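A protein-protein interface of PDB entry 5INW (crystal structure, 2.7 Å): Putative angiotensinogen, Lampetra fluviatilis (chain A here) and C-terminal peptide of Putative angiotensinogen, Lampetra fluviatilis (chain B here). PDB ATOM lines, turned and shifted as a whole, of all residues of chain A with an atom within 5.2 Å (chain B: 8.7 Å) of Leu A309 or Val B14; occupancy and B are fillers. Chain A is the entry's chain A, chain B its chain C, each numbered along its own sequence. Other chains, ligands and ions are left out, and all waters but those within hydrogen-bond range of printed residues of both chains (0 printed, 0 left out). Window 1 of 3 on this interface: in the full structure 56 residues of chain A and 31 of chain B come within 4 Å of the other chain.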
ATOM      1  N   PHE A 107      -1.207  -1.200  13.909  1.00  0.00           N
ATOM      2  CA  PHE A 107      -0.070  -1.627  13.073  1.00  0.00           C
ATOM      3  C   PHE A 107       0.621  -2.873  13.582  1.00  0.00           C
ATOM      4  O   PHE A 107       1.070  -2.931  14.708  1.00  0.00           O
ATOM      5  CB  PHE A 107       0.956  -0.523  12.933  1.00  0.00           C
ATOM      6  CG  PHE A 107       1.796  -0.690  11.725  1.00  0.00           C
ATOM      7  CD1 PHE A 107       1.221  -0.660  10.476  1.00  0.00           C
ATOM      8  CD2 PHE A 107       3.173  -0.893  11.818  1.00  0.00           C
ATOM      9  CE1 PHE A 107       1.991  -0.815   9.338  1.00  0.00           C
ATOM     10  CE2 PHE A 107       3.939  -1.092  10.689  1.00  0.00           C
ATOM     11  CZ  PHE A 107       3.350  -1.043   9.445  1.00  0.00           C
ATOM     12  N   VAL A 297      -9.592   3.891  -2.705  1.00  0.00           N
ATOM     13  CA  VAL A 297      -8.469   2.932  -2.656  1.00  0.00           C
ATOM     14  C   VAL A 297      -7.363   3.365  -3.611  1.00  0.00           C
ATOM     15  O   VAL A 297      -7.645   3.729  -4.749  1.00  0.00           O
ATOM     16  CB  VAL A 297      -8.937   1.516  -3.069  1.00  0.00           C
ATOM     17  CG1 VAL A 297      -7.758   0.527  -3.118  1.00  0.00           C
ATOM     18  CG2 VAL A 297     -10.029   1.028  -2.119  1.00  0.00           C
ATOM     19  N   VAL A 298      -6.104   3.253  -3.179  1.00  0.00           N
ATOM     20  CA  VAL A 298      -4.953   3.608  -4.015  1.00  0.00           C
ATOM     21  C   VAL A 298      -3.768   2.714  -3.743  1.00  0.00           C
ATOM     22  O   VAL A 298      -3.500   2.372  -2.602  1.00  0.00           O
ATOM     23  CB  VAL A 298      -4.563   5.102  -3.819  1.00  0.00           C
ATOM     24  CG1 VAL A 298      -4.178   5.425  -2.391  1.00  0.00           C
ATOM     25  CG2 VAL A 298      -3.423   5.518  -4.733  1.00  0.00           C
ATOM     26  N   LYS A 299      -3.033   2.400  -4.803  1.00  0.00           N
ATOM     27  CA  LYS A 299      -1.885   1.510  -4.768  1.00  0.00           C
ATOM     28  C   LYS A 299      -0.640   2.342  -4.943  1.00  0.00           C
ATOM     29  O   LYS A 299      -0.451   2.942  -5.985  1.00  0.00           O
ATOM     30  CB  LYS A 299      -2.001   0.492  -5.896  1.00  0.00           C
ATOM     31  CG  LYS A 299      -0.874  -0.511  -6.062  1.00  0.00           C
ATOM     32  CD  LYS A 299      -1.324  -1.624  -7.016  1.00  0.00           C
ATOM     33  CE  LYS A 299      -0.211  -2.617  -7.401  1.00  0.00           C
ATOM     34  NZ  LYS A 299       0.822  -2.084  -8.360  1.00  0.00           N
ATOM     35  N   LEU A 300       0.228   2.337  -3.942  1.00  0.00           N
ATOM     36  CA  LEU A 300       1.503   3.041  -4.003  1.00  0.00           C
ATOM     37  C   LEU A 300       2.626   2.045  -4.163  1.00  0.00           C
ATOM     38  O   LEU A 300       3.100   1.490  -3.190  1.00  0.00           O
ATOM     39  CB  LEU A 300       1.735   3.918  -2.760  1.00  0.00           C
ATOM     40  CG  LEU A 300       0.480   4.705  -2.439  1.00  0.00           C
ATOM     41  CD1 LEU A 300       0.596   5.432  -1.099  1.00  0.00           C
ATOM     42  CD2 LEU A 300       0.123   5.640  -3.568  1.00  0.00           C
ATOM     43  N   SER A 307       3.981  -3.146  -2.719  1.00  0.00           N
ATOM     44  CA  SER A 307       3.325  -1.863  -2.702  1.00  0.00           C
ATOM     45  C   SER A 307       2.484  -1.688  -1.449  1.00  0.00           C
ATOM     46  O   SER A 307       2.232  -2.639  -0.744  1.00  0.00           O
ATOM     47  CB  SER A 307       2.553  -1.614  -4.016  1.00  0.00           C
ATOM     48  OG  SER A 307       1.561  -2.561  -4.204  1.00  0.00           O
ATOM     49  N   MET A 308       2.152  -0.427  -1.159  1.00  0.00           N
ATOM     50  CA  MET A 308       1.243  -0.101  -0.095  1.00  0.00           C
ATOM     51  C   MET A 308      -0.101   0.227  -0.705  1.00  0.00           C
ATOM     52  O   MET A 308      -0.206   1.084  -1.557  1.00  0.00           O
ATOM     53  CB  MET A 308       1.731   1.088   0.718  1.00  0.00           C
ATOM     54  CG  MET A 308       0.836   1.446   1.909  1.00  0.00           C
ATOM     55  SD  MET A 308       1.329   2.999   2.726  1.00  0.00           S
ATOM     56  CE  MET A 308       2.669   2.429   3.749  1.00  0.00           C
ATOM     57  N   LEU A 309      -1.117  -0.464  -0.228  1.00  0.00           N
ATOM     58  CA  LEU A 309      -2.499  -0.133  -0.478  1.00  0.00           C
ATOM     59  C   LEU A 309      -2.955   0.826   0.567  1.00  0.00           C
ATOM     60  O   LEU A 309      -2.792   0.507   1.760  1.00  0.00           O
ATOM     61  CB  LEU A 309      -3.390  -1.371  -0.318  1.00  0.00           C
ATOM     62  CG  LEU A 309      -3.831  -2.104  -1.579  1.00  0.00           C
ATOM     63  CD1 LEU A 309      -5.152  -2.779  -1.243  1.00  0.00           C
ATOM     64  CD2 LEU A 309      -3.979  -1.196  -2.808  1.00  0.00           C
ATOM     65  N   VAL A 310      -3.555   1.962   0.153  1.00  0.00           N
ATOM     66  CA  VAL A 310      -4.139   2.934   1.104  1.00  0.00           C
ATOM     67  C   VAL A 310      -5.632   3.081   0.855  1.00  0.00           C
ATOM     68  O   VAL A 310      -6.045   3.428  -0.236  1.00  0.00           O
ATOM     69  CB  VAL A 310      -3.434   4.299   1.078  1.00  0.00           C
ATOM     70  CG1 VAL A 310      -4.159   5.306   1.956  1.00  0.00           C
ATOM     71  CG2 VAL A 310      -2.005   4.155   1.553  1.00  0.00           C
ATOM     72  N   ILE A 311      -6.420   2.810   1.892  1.00  0.00           N
ATOM     73  CA  ILE A 311      -7.884   2.892   1.828  1.00  0.00           C
ATOM     74  C   ILE A 311      -8.381   4.006   2.752  1.00  0.00           C
ATOM     75  O   ILE A 311      -8.205   3.909   3.975  1.00  0.00           O
ATOM     76  CB  ILE A 311      -8.545   1.552   2.202  1.00  0.00           C
ATOM     77  CG1 ILE A 311      -7.987   0.405   1.350  1.00  0.00           C
ATOM     78  CG2 ILE A 311     -10.045   1.618   2.030  1.00  0.00           C
ATOM     79  CD1 ILE A 311      -6.948  -0.394   2.091  1.00  0.00           C
ATOM     80  N   LEU A 331      -9.401  -8.225   0.020  1.00  0.00           N
ATOM     81  CA  LEU A 331      -8.128  -7.847  -0.574  1.00  0.00           C
ATOM     82  C   LEU A 331      -8.117  -8.157  -2.056  1.00  0.00           C
ATOM     83  O   LEU A 331      -7.740  -7.307  -2.865  1.00  0.00           O
ATOM     84  CB  LEU A 331      -6.953  -8.538   0.128  1.00  0.00           C
ATOM     85  CG  LEU A 331      -5.555  -8.382  -0.511  1.00  0.00           C
ATOM     86  CD1 LEU A 331      -5.174  -6.913  -0.519  1.00  0.00           C
ATOM     87  CD2 LEU A 331      -4.529  -9.222   0.216  1.00  0.00           C
ATOM     88  N   TRP A 334     -10.411  -5.530  -3.807  1.00  0.00           N
ATOM     89  CA  TRP A 334      -9.709  -4.246  -3.997  1.00  0.00           C
ATOM     90  C   TRP A 334      -8.625  -4.248  -5.064  1.00  0.00           C
ATOM     91  O   TRP A 334      -8.437  -3.232  -5.726  1.00  0.00           O
ATOM     92  CB  TRP A 334      -9.068  -3.786  -2.692  1.00  0.00           C
ATOM     93  CG  TRP A 334     -10.021  -3.186  -1.718  1.00  0.00           C
ATOM     94  CD1 TRP A 334     -11.155  -2.504  -2.010  1.00  0.00           C
ATOM     95  CD2 TRP A 334      -9.890  -3.151  -0.284  1.00  0.00           C
ATOM     96  NE1 TRP A 334     -11.760  -2.085  -0.862  1.00  0.00           N
ATOM     97  CE2 TRP A 334     -11.007  -2.465   0.215  1.00  0.00           C
ATOM     98  CE3 TRP A 334      -8.953  -3.647   0.617  1.00  0.00           C
ATOM     99  CZ2 TRP A 334     -11.215  -2.259   1.580  1.00  0.00           C
ATOM    100  CZ3 TRP A 334      -9.165  -3.441   1.992  1.00  0.00           C
ATOM    101  CH2 TRP A 334     -10.285  -2.756   2.451  1.00  0.00           C
ATOM    102  N   LEU A 335      -7.935  -5.387  -5.227  1.00  0.00           N
ATOM    103  CA  LEU A 335      -6.877  -5.547  -6.241  1.00  0.00           C
ATOM    104  C   LEU A 335      -7.394  -5.759  -7.663  1.00  0.00           C
ATOM    105  O   LEU A 335      -6.752  -5.351  -8.622  1.00  0.00           O
ATOM    106  CB  LEU A 335      -5.978  -6.715  -5.892  1.00  0.00           C
ATOM    107  CG  LEU A 335      -5.109  -6.484  -4.678  1.00  0.00           C
ATOM    108  CD1 LEU A 335      -4.643  -7.821  -4.126  1.00  0.00           C
ATOM    109  CD2 LEU A 335      -3.930  -5.584  -5.034  1.00  0.00           C
ATOM    110  N   LEU A 338      -8.808  -2.268  -8.825  1.00  0.00           N
ATOM    111  CA  LEU A 338      -7.666  -1.488  -9.327  1.00  0.00           C
ATOM    112  C   LEU A 338      -7.281  -1.872 -10.757  1.00  0.00           C
ATOM    113  O   LEU A 338      -6.873  -3.015 -11.007  1.00  0.00           O
ATOM    114  CB  LEU A 338      -6.432  -1.675  -8.422  1.00  0.00           C
ATOM    115  CG  LEU A 338      -6.577  -1.010  -7.061  1.00  0.00           C
ATOM    116  CD1 LEU A 338      -5.558  -1.552  -6.082  1.00  0.00           C
ATOM    117  CD2 LEU A 338      -6.451   0.498  -7.168  1.00  0.00           C
ATOM    118  N   LEU A 399       6.085   2.216  11.802  1.00  0.00           N
ATOM    119  CA  LEU A 399       5.843   2.587  10.413  1.00  0.00           C
ATOM    120  C   LEU A 399       6.361   3.992  10.204  1.00  0.00           C
ATOM    121  O   LEU A 399       5.991   4.872  10.930  1.00  0.00           O
ATOM    122  CB  LEU A 399       4.345   2.495  10.049  1.00  0.00           C
ATOM    123  CG  LEU A 399       4.014   2.926   8.609  1.00  0.00           C
ATOM    124  CD1 LEU A 399       4.789   2.098   7.578  1.00  0.00           C
ATOM    125  CD2 LEU A 399       2.513   2.858   8.342  1.00  0.00           C
ATOM    126  N   VAL B   8      -5.227  11.922   1.260  1.00  0.00           N
ATOM    127  CA  VAL B   8      -5.244  11.143   2.455  1.00  0.00           C
ATOM    128  C   VAL B   8      -5.160  12.199   3.543  1.00  0.00           C
ATOM    129  O   VAL B   8      -4.069  12.531   4.011  1.00  0.00           O
ATOM    130  CB  VAL B   8      -4.065  10.136   2.468  1.00  0.00           C
ATOM    131  CG1 VAL B   8      -4.149   9.189   3.677  1.00  0.00           C
ATOM    132  CG2 VAL B   8      -4.035   9.352   1.148  1.00  0.00           C
ATOM    133  N   PRO B  11      -8.504   9.446   8.545  1.00  0.00           N
ATOM    134  CA  PRO B  11      -8.001   8.140   8.882  1.00  0.00           C
ATOM    135  C   PRO B  11      -8.108   7.191   7.722  1.00  0.00           C
ATOM    136  O   PRO B  11      -9.092   7.249   6.980  1.00  0.00           O
ATOM    137  CB  PRO B  11      -8.914   7.700   9.993  1.00  0.00           C
ATOM    138  CG  PRO B  11      -9.353   8.948  10.647  1.00  0.00           C
ATOM    139  CD  PRO B  11      -9.069  10.092   9.729  1.00  0.00           C
ATOM    140  N   PHE B  12      -7.087   6.344   7.573  1.00  0.00           N
ATOM    141  CA  PHE B  12      -7.013   5.400   6.474  1.00  0.00           C
ATOM    142  C   PHE B  12      -6.445   4.041   6.877  1.00  0.00           C
ATOM    143  O   PHE B  12      -5.648   3.930   7.788  1.00  0.00           O
ATOM    144  CB  PHE B  12      -6.208   5.991   5.343  1.00  0.00           C
ATOM    145  CG  PHE B  12      -4.775   6.196   5.655  1.00  0.00           C
ATOM    146  CD1 PHE B  12      -3.830   5.261   5.285  1.00  0.00           C
ATOM    147  CD2 PHE B  12      -4.349   7.355   6.263  1.00  0.00           C
ATOM    148  CE1 PHE B  12      -2.485   5.489   5.530  1.00  0.00           C
ATOM    149  CE2 PHE B  12      -3.003   7.594   6.508  1.00  0.00           C
ATOM    150  CZ  PHE B  12      -2.077   6.670   6.152  1.00  0.00           C
ATOM    151  N   VAL B  13      -6.889   3.005   6.180  1.00  0.00           N
ATOM    152  CA  VAL B  13      -6.328   1.675   6.299  1.00  0.00           C
ATOM    153  C   VAL B  13      -5.113   1.523   5.368  1.00  0.00           C
ATOM    154  O   VAL B  13      -5.081   2.040   4.229  1.00  0.00           O
ATOM    155  CB  VAL B  13      -7.372   0.619   5.954  1.00  0.00           C
ATOM    156  CG1 VAL B  13      -6.794  -0.793   6.018  1.00  0.00           C
ATOM    157  CG2 VAL B  13      -8.545   0.747   6.905  1.00  0.00           C
ATOM    158  N   VAL B  14      -4.120   0.781   5.853  1.00  0.00           N
ATOM    159  CA  VAL B  14      -2.833   0.700   5.193  1.00  0.00           C
ATOM    160  C   VAL B  14      -2.434  -0.784   5.161  1.00  0.00           C
ATOM    161  O   VAL B  14      -2.680  -1.489   6.102  1.00  0.00           O
ATOM    162  CB  VAL B  14      -1.827   1.634   5.906  1.00  0.00           C
ATOM    163  CG1 VAL B  14      -1.238   0.978   7.126  1.00  0.00           C
ATOM    164  CG2 VAL B  14      -0.738   2.070   4.983  1.00  0.00           C
ATOM    165  N   LEU B  15      -1.931  -1.254   4.023  1.00  0.00           N
ATOM    166  CA  LEU B  15      -1.486  -2.636   3.841  1.00  0.00           C
ATOM    167  C   LEU B  15      -0.234  -2.645   2.969  1.00  0.00           C
ATOM    168  O   LEU B  15      -0.249  -2.124   1.875  1.00  0.00           O
ATOM    169  CB  LEU B  15      -2.547  -3.514   3.156  1.00  0.00           C
ATOM    170  CG  LEU B  15      -3.939  -3.624   3.778  1.00  0.00           C
ATOM    171  CD1 LEU B  15      -4.765  -4.524   2.890  1.00  0.00           C
ATOM    172  CD2 LEU B  15      -3.956  -4.173   5.190  1.00  0.00           C
ATOM    173  N   ILE B  16       0.828  -3.260   3.464  1.00  0.00           N
ATOM    174  CA  ILE B  16       2.059  -3.375   2.743  1.00  0.00           C
ATOM    175  C   ILE B  16       2.116  -4.834   2.333  1.00  0.00           C
ATOM    176  O   ILE B  16       2.083  -5.708   3.202  1.00  0.00           O
ATOM    177  CB  ILE B  16       3.224  -2.991   3.656  1.00  0.00           C
ATOM    178  CG1 ILE B  16       3.211  -1.498   3.901  1.00  0.00           C
ATOM    179  CG2 ILE B  16       4.544  -3.387   3.025  1.00  0.00           C
ATOM    180  CD1 ILE B  16       4.135  -1.058   4.992  1.00  0.00           C
ATOM    181  N   TYR B  17       2.203  -5.117   1.034  1.00  0.00           N
ATOM    182  CA  TYR B  17       2.051  -6.493   0.569  1.00  0.00           C
ATOM    183  C   TYR B  17       2.915  -6.838  -0.633  1.00  0.00           C
ATOM    184  O   TYR B  17       3.287  -5.967  -1.400  1.00  0.00           O
ATOM    185  CB  TYR B  17       0.578  -6.725   0.236  1.00  0.00           C
ATOM    186  CG  TYR B  17       0.158  -6.056  -1.044  1.00  0.00           C
ATOM    187  CD1 TYR B  17      -0.141  -4.670  -1.101  1.00  0.00           C
ATOM    188  CD2 TYR B  17       0.106  -6.792  -2.225  1.00  0.00           C
ATOM    189  CE1 TYR B  17      -0.501  -4.070  -2.313  1.00  0.00           C
ATOM    190  CE2 TYR B  17      -0.251  -6.201  -3.427  1.00  0.00           C
ATOM    191  CZ  TYR B  17      -0.551  -4.852  -3.490  1.00  0.00           C
ATOM    192  OH  TYR B  17      -0.881  -4.344  -4.756  1.00  0.00           O
ATOM    193  N   VAL B  24       0.489 -10.272   2.817  1.00  0.00           N
ATOM    194  CA  VAL B  24       0.446  -9.059   3.584  1.00  0.00           C
ATOM    195  C   VAL B  24       1.457  -9.152   4.701  1.00  0.00           C
ATOM    196  O   VAL B  24       1.433 -10.065   5.527  1.00  0.00           O
ATOM    197  CB  VAL B  24      -0.922  -8.812   4.131  1.00  0.00           C
ATOM    198  CG1 VAL B  24      -0.895  -7.538   4.968  1.00  0.00           C
ATOM    199  CG2 VAL B  24      -1.863  -8.707   2.971  1.00  0.00           C
ATOM    200  N   ILE B  25       2.309  -8.152   4.728  1.00  0.00           N
ATOM    201  CA  ILE B  25       3.444  -8.104   5.592  1.00  0.00           C
ATOM    202  C   ILE B  25       3.184  -7.222   6.800  1.00  0.00           C
ATOM    203  O   ILE B  25       3.667  -7.542   7.878  1.00  0.00           O
ATOM    204  CB  ILE B  25       4.646  -7.561   4.799  1.00  0.00           C
ATOM    205  CG1 ILE B  25       4.823  -8.414   3.551  1.00  0.00           C
ATOM    206  CG2 ILE B  25       5.933  -7.592   5.634  1.00  0.00           C
ATOM    207  CD1 ILE B  25       5.801  -7.829   2.592  1.00  0.00           C
ATOM    208  N   PHE B  26       2.529  -6.079   6.588  1.00  0.00           N
ATOM    209  CA  PHE B  26       2.040  -5.239   7.655  1.00  0.00           C
ATOM    210  C   PHE B  26       0.640  -4.829   7.321  1.00  0.00           C
ATOM    211  O   PHE B  26       0.306  -4.697   6.169  1.00  0.00           O
ATOM    212  CB  PHE B  26       2.864  -3.959   7.800  1.00  0.00           C
ATOM    213  CG  PHE B  26       4.302  -4.185   8.192  1.00  0.00           C
ATOM    214  CD1 PHE B  26       4.663  -4.222   9.527  1.00  0.00           C
ATOM    215  CD2 PHE B  26       5.278  -4.393   7.223  1.00  0.00           C
ATOM    216  CE1 PHE B  26       5.982  -4.453   9.888  1.00  0.00           C
ATOM    217  CE2 PHE B  26       6.574  -4.659   7.585  1.00  0.00           C
ATOM    218  CZ  PHE B  26       6.932  -4.677   8.916  1.00  0.00           C
ATOM    219  N   MET B  27      -0.178  -4.683   8.356  1.00  0.00           N
ATOM    220  CA  MET B  27      -1.543  -4.245   8.262  1.00  0.00           C
ATOM    221  C   MET B  27      -1.726  -3.185   9.273  1.00  0.00           C
ATOM    222  O   MET B  27      -1.189  -3.254  10.386  1.00  0.00           O
ATOM    223  CB  MET B  27      -2.510  -5.347   8.710  1.00  0.00           C
ATOM    224  CG  MET B  27      -2.716  -6.432   7.704  1.00  0.00           C
ATOM    225  SD  MET B  27      -3.530  -7.896   8.289  1.00  0.00           S
ATOM    226  CE  MET B  27      -4.779  -7.175   9.289  1.00  0.00           C
ATOM    227  N   GLY B  28      -2.599  -2.252   8.950  1.00  0.00           N
ATOM    228  CA  GLY B  28      -3.040  -1.312   9.955  1.00  0.00           C
ATOM    229  C   GLY B  28      -3.945  -0.196   9.492  1.00  0.00           C
ATOM    230  O   GLY B  28      -4.470  -0.194   8.365  1.00  0.00           O
ATOM    231  N   ARG B  29      -4.105   0.747  10.425  1.00  0.00           N
ATOM    232  CA  ARG B  29      -4.885   1.940  10.262  1.00  0.00           C
ATOM    233  C   ARG B  29      -4.095   3.074  10.879  1.00  0.00           C
ATOM    234  O   ARG B  29      -3.665   2.989  12.040  1.00  0.00           O
ATOM    235  CB  ARG B  29      -6.250   1.814  10.953  1.00  0.00           C
ATOM    236  CG  ARG B  29      -7.043   3.138  11.079  1.00  0.00           C
ATOM    237  CD  ARG B  29      -7.411   3.441  12.515  1.00  0.00           C
ATOM    238  NE  ARG B  29      -8.508   2.562  12.901  1.00  0.00           N
ATOM    239  CZ  ARG B  29      -9.074   2.512  14.097  1.00  0.00           C
ATOM    240  NH1 ARG B  29     -10.093   1.693  14.273  1.00  0.00           N
ATOM    241  NH2 ARG B  29      -8.631   3.269  15.103  1.00  0.00           N
ATOM    242  N   VAL B  30      -3.924   4.130  10.083  1.00  0.00           N
ATOM    243  CA  VAL B  30      -3.314   5.350  10.557  1.00  0.00           C
ATOM    244  C   VAL B  30      -4.406   6.384  10.798  1.00  0.00           C
ATOM    245  O   VAL B  30      -5.080   6.795   9.848  1.00  0.00           O
ATOM    246  CB  VAL B  30      -2.299   5.892   9.557  1.00  0.00           C
ATOM    247  CG1 VAL B  30      -1.692   7.160  10.108  1.00  0.00           C
ATOM    248  CG2 VAL B  30      -1.215   4.860   9.311  1.00  0.00           C
ATOM    249  N   ALA B  31      -4.581   6.754  12.074  1.00  0.00           N
ATOM    250  CA  ALA B  31      -5.505   7.809  12.503  1.00  0.00           C
ATOM    251  C   ALA B  31      -4.845   9.044  13.143  1.00  0.00           C
ATOM    252  O   ALA B  31      -5.484  10.067  13.224  1.00  0.00           O
ATOM    253  CB  ALA B  31      -6.532   7.241  13.445  1.00  0.00           C
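O of Ser A307 lies within hydrogen-bond range of N of Tyr B17 (3.1 Å).
The backbone carbonyl oxygen (O) of Leu B15 lies within hydrogen-bond range of the backbone NH (N) of Leu A309 (2.8 Å).
The backbone carbonyl oxygen (O) of Ile A311 lies within hydrogen-bond range of the backbone NH (N) of Val B13 (2.7 Å).
The backbone NH of Val A310 lies within hydrogen-bond range of the backbone carbonyl oxygen of Val A298, 2.8 Å away.
The backbone NH of Leu A300 lies within hydrogen-bond range of the backbone carbonyl oxygen of Met A308 (2.7 Å).
The backbone carbonyl oxygen (O) of Phe B12 sits at hydrogen-bond distance from the backbone NH (N) of Val B30, 2.9 Å away.
The backbone NH of Val B14 lies within hydrogen-bond range of the backbone carbonyl oxygen of Gly B28.
The backbone NH of Ile B25 is in hydrogen-bond range of the backbone carbonyl oxygen of Ile B16 (2.9 Å).
N of Ile B16 is in hydrogen-bond range of O of Phe B26.
CZ of Phe A107 touches CB of Phe B26 (3.4 Å).
O of Met B27 touches CA of Phe A107, 3.3 Å away.
Val B14 touches Met A308.
Leu A309 touches Val B13 (O to O, 3.7 Å).
CA of Val B14 touches O of Leu A309, at 3.4 Å.
CE1 of Tyr B17 touches CG of Leu A309 (3.9 Å).
Phe B12 touches Val A310.
Val B13 touches Val A310 (O to CA, 3.4 Å).
O of Ile A311 touches CA of Phe B12 (3.1 Å).
CD2 of Leu A335 touches OH of Tyr B17 (3.3 Å).
Printed residues of chain B within 4 Å of Lys A299: Tyr B17 (3.2 Å).
Printed residues of chain B within 4 Å of Ser A307: Leu B15 (3.6 Å), Ile B16 (3.6 Å) and Tyr B17 (3.1 Å).
Met A308 touches just these residues of chain B: Val B14 (3.2 Å), Leu B15 (3.2 Å) and Ile B16 (3.97 Å).
Leu A309 touches just these residues of chain B: Val B13 (3.7 Å), Val B14 (3.4 Å), Leu B15 (2.8 Å) and Tyr B17 (3.9 Å).
Val B14 touches just these residues of chain A: Met A308 and Leu A309.
The nearest residue of chain B that does not touch Leu A309 is Ile B16 (5.0 Å).
The nearest residue of chain A that does not touch Val B14 is Val A310 (4.2 Å).
The nearest printed residue of chain B that does not touch Leu A335 is Val B24 (7.7 Å).
Of the 16 printed residues of chain B, 9 touch a printed residue of chain A.
Hydrophobic or aromatic side chains of chain B that line the printed part of chain A: Phe B12, Val B13, Val B14, Ile B16, Tyr B17, Val B24 and Phe B26.
Along chain B the printed residues that touch a printed residue of chain A span positions 12 to 27.
Hydrophobic or aromatic side chains of chain A that line the printed part of chain B: Phe A107, Met A308, Leu A309, Val A310, Ile A311, Leu A331 and Leu A335.
Among the printed residues, 19 pairs touch across the chains.
Among the printed residues, no Asp or Glu carboxylate lies within 4 Å of a Lys or Arg side-chain nitrogen of the other chain.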
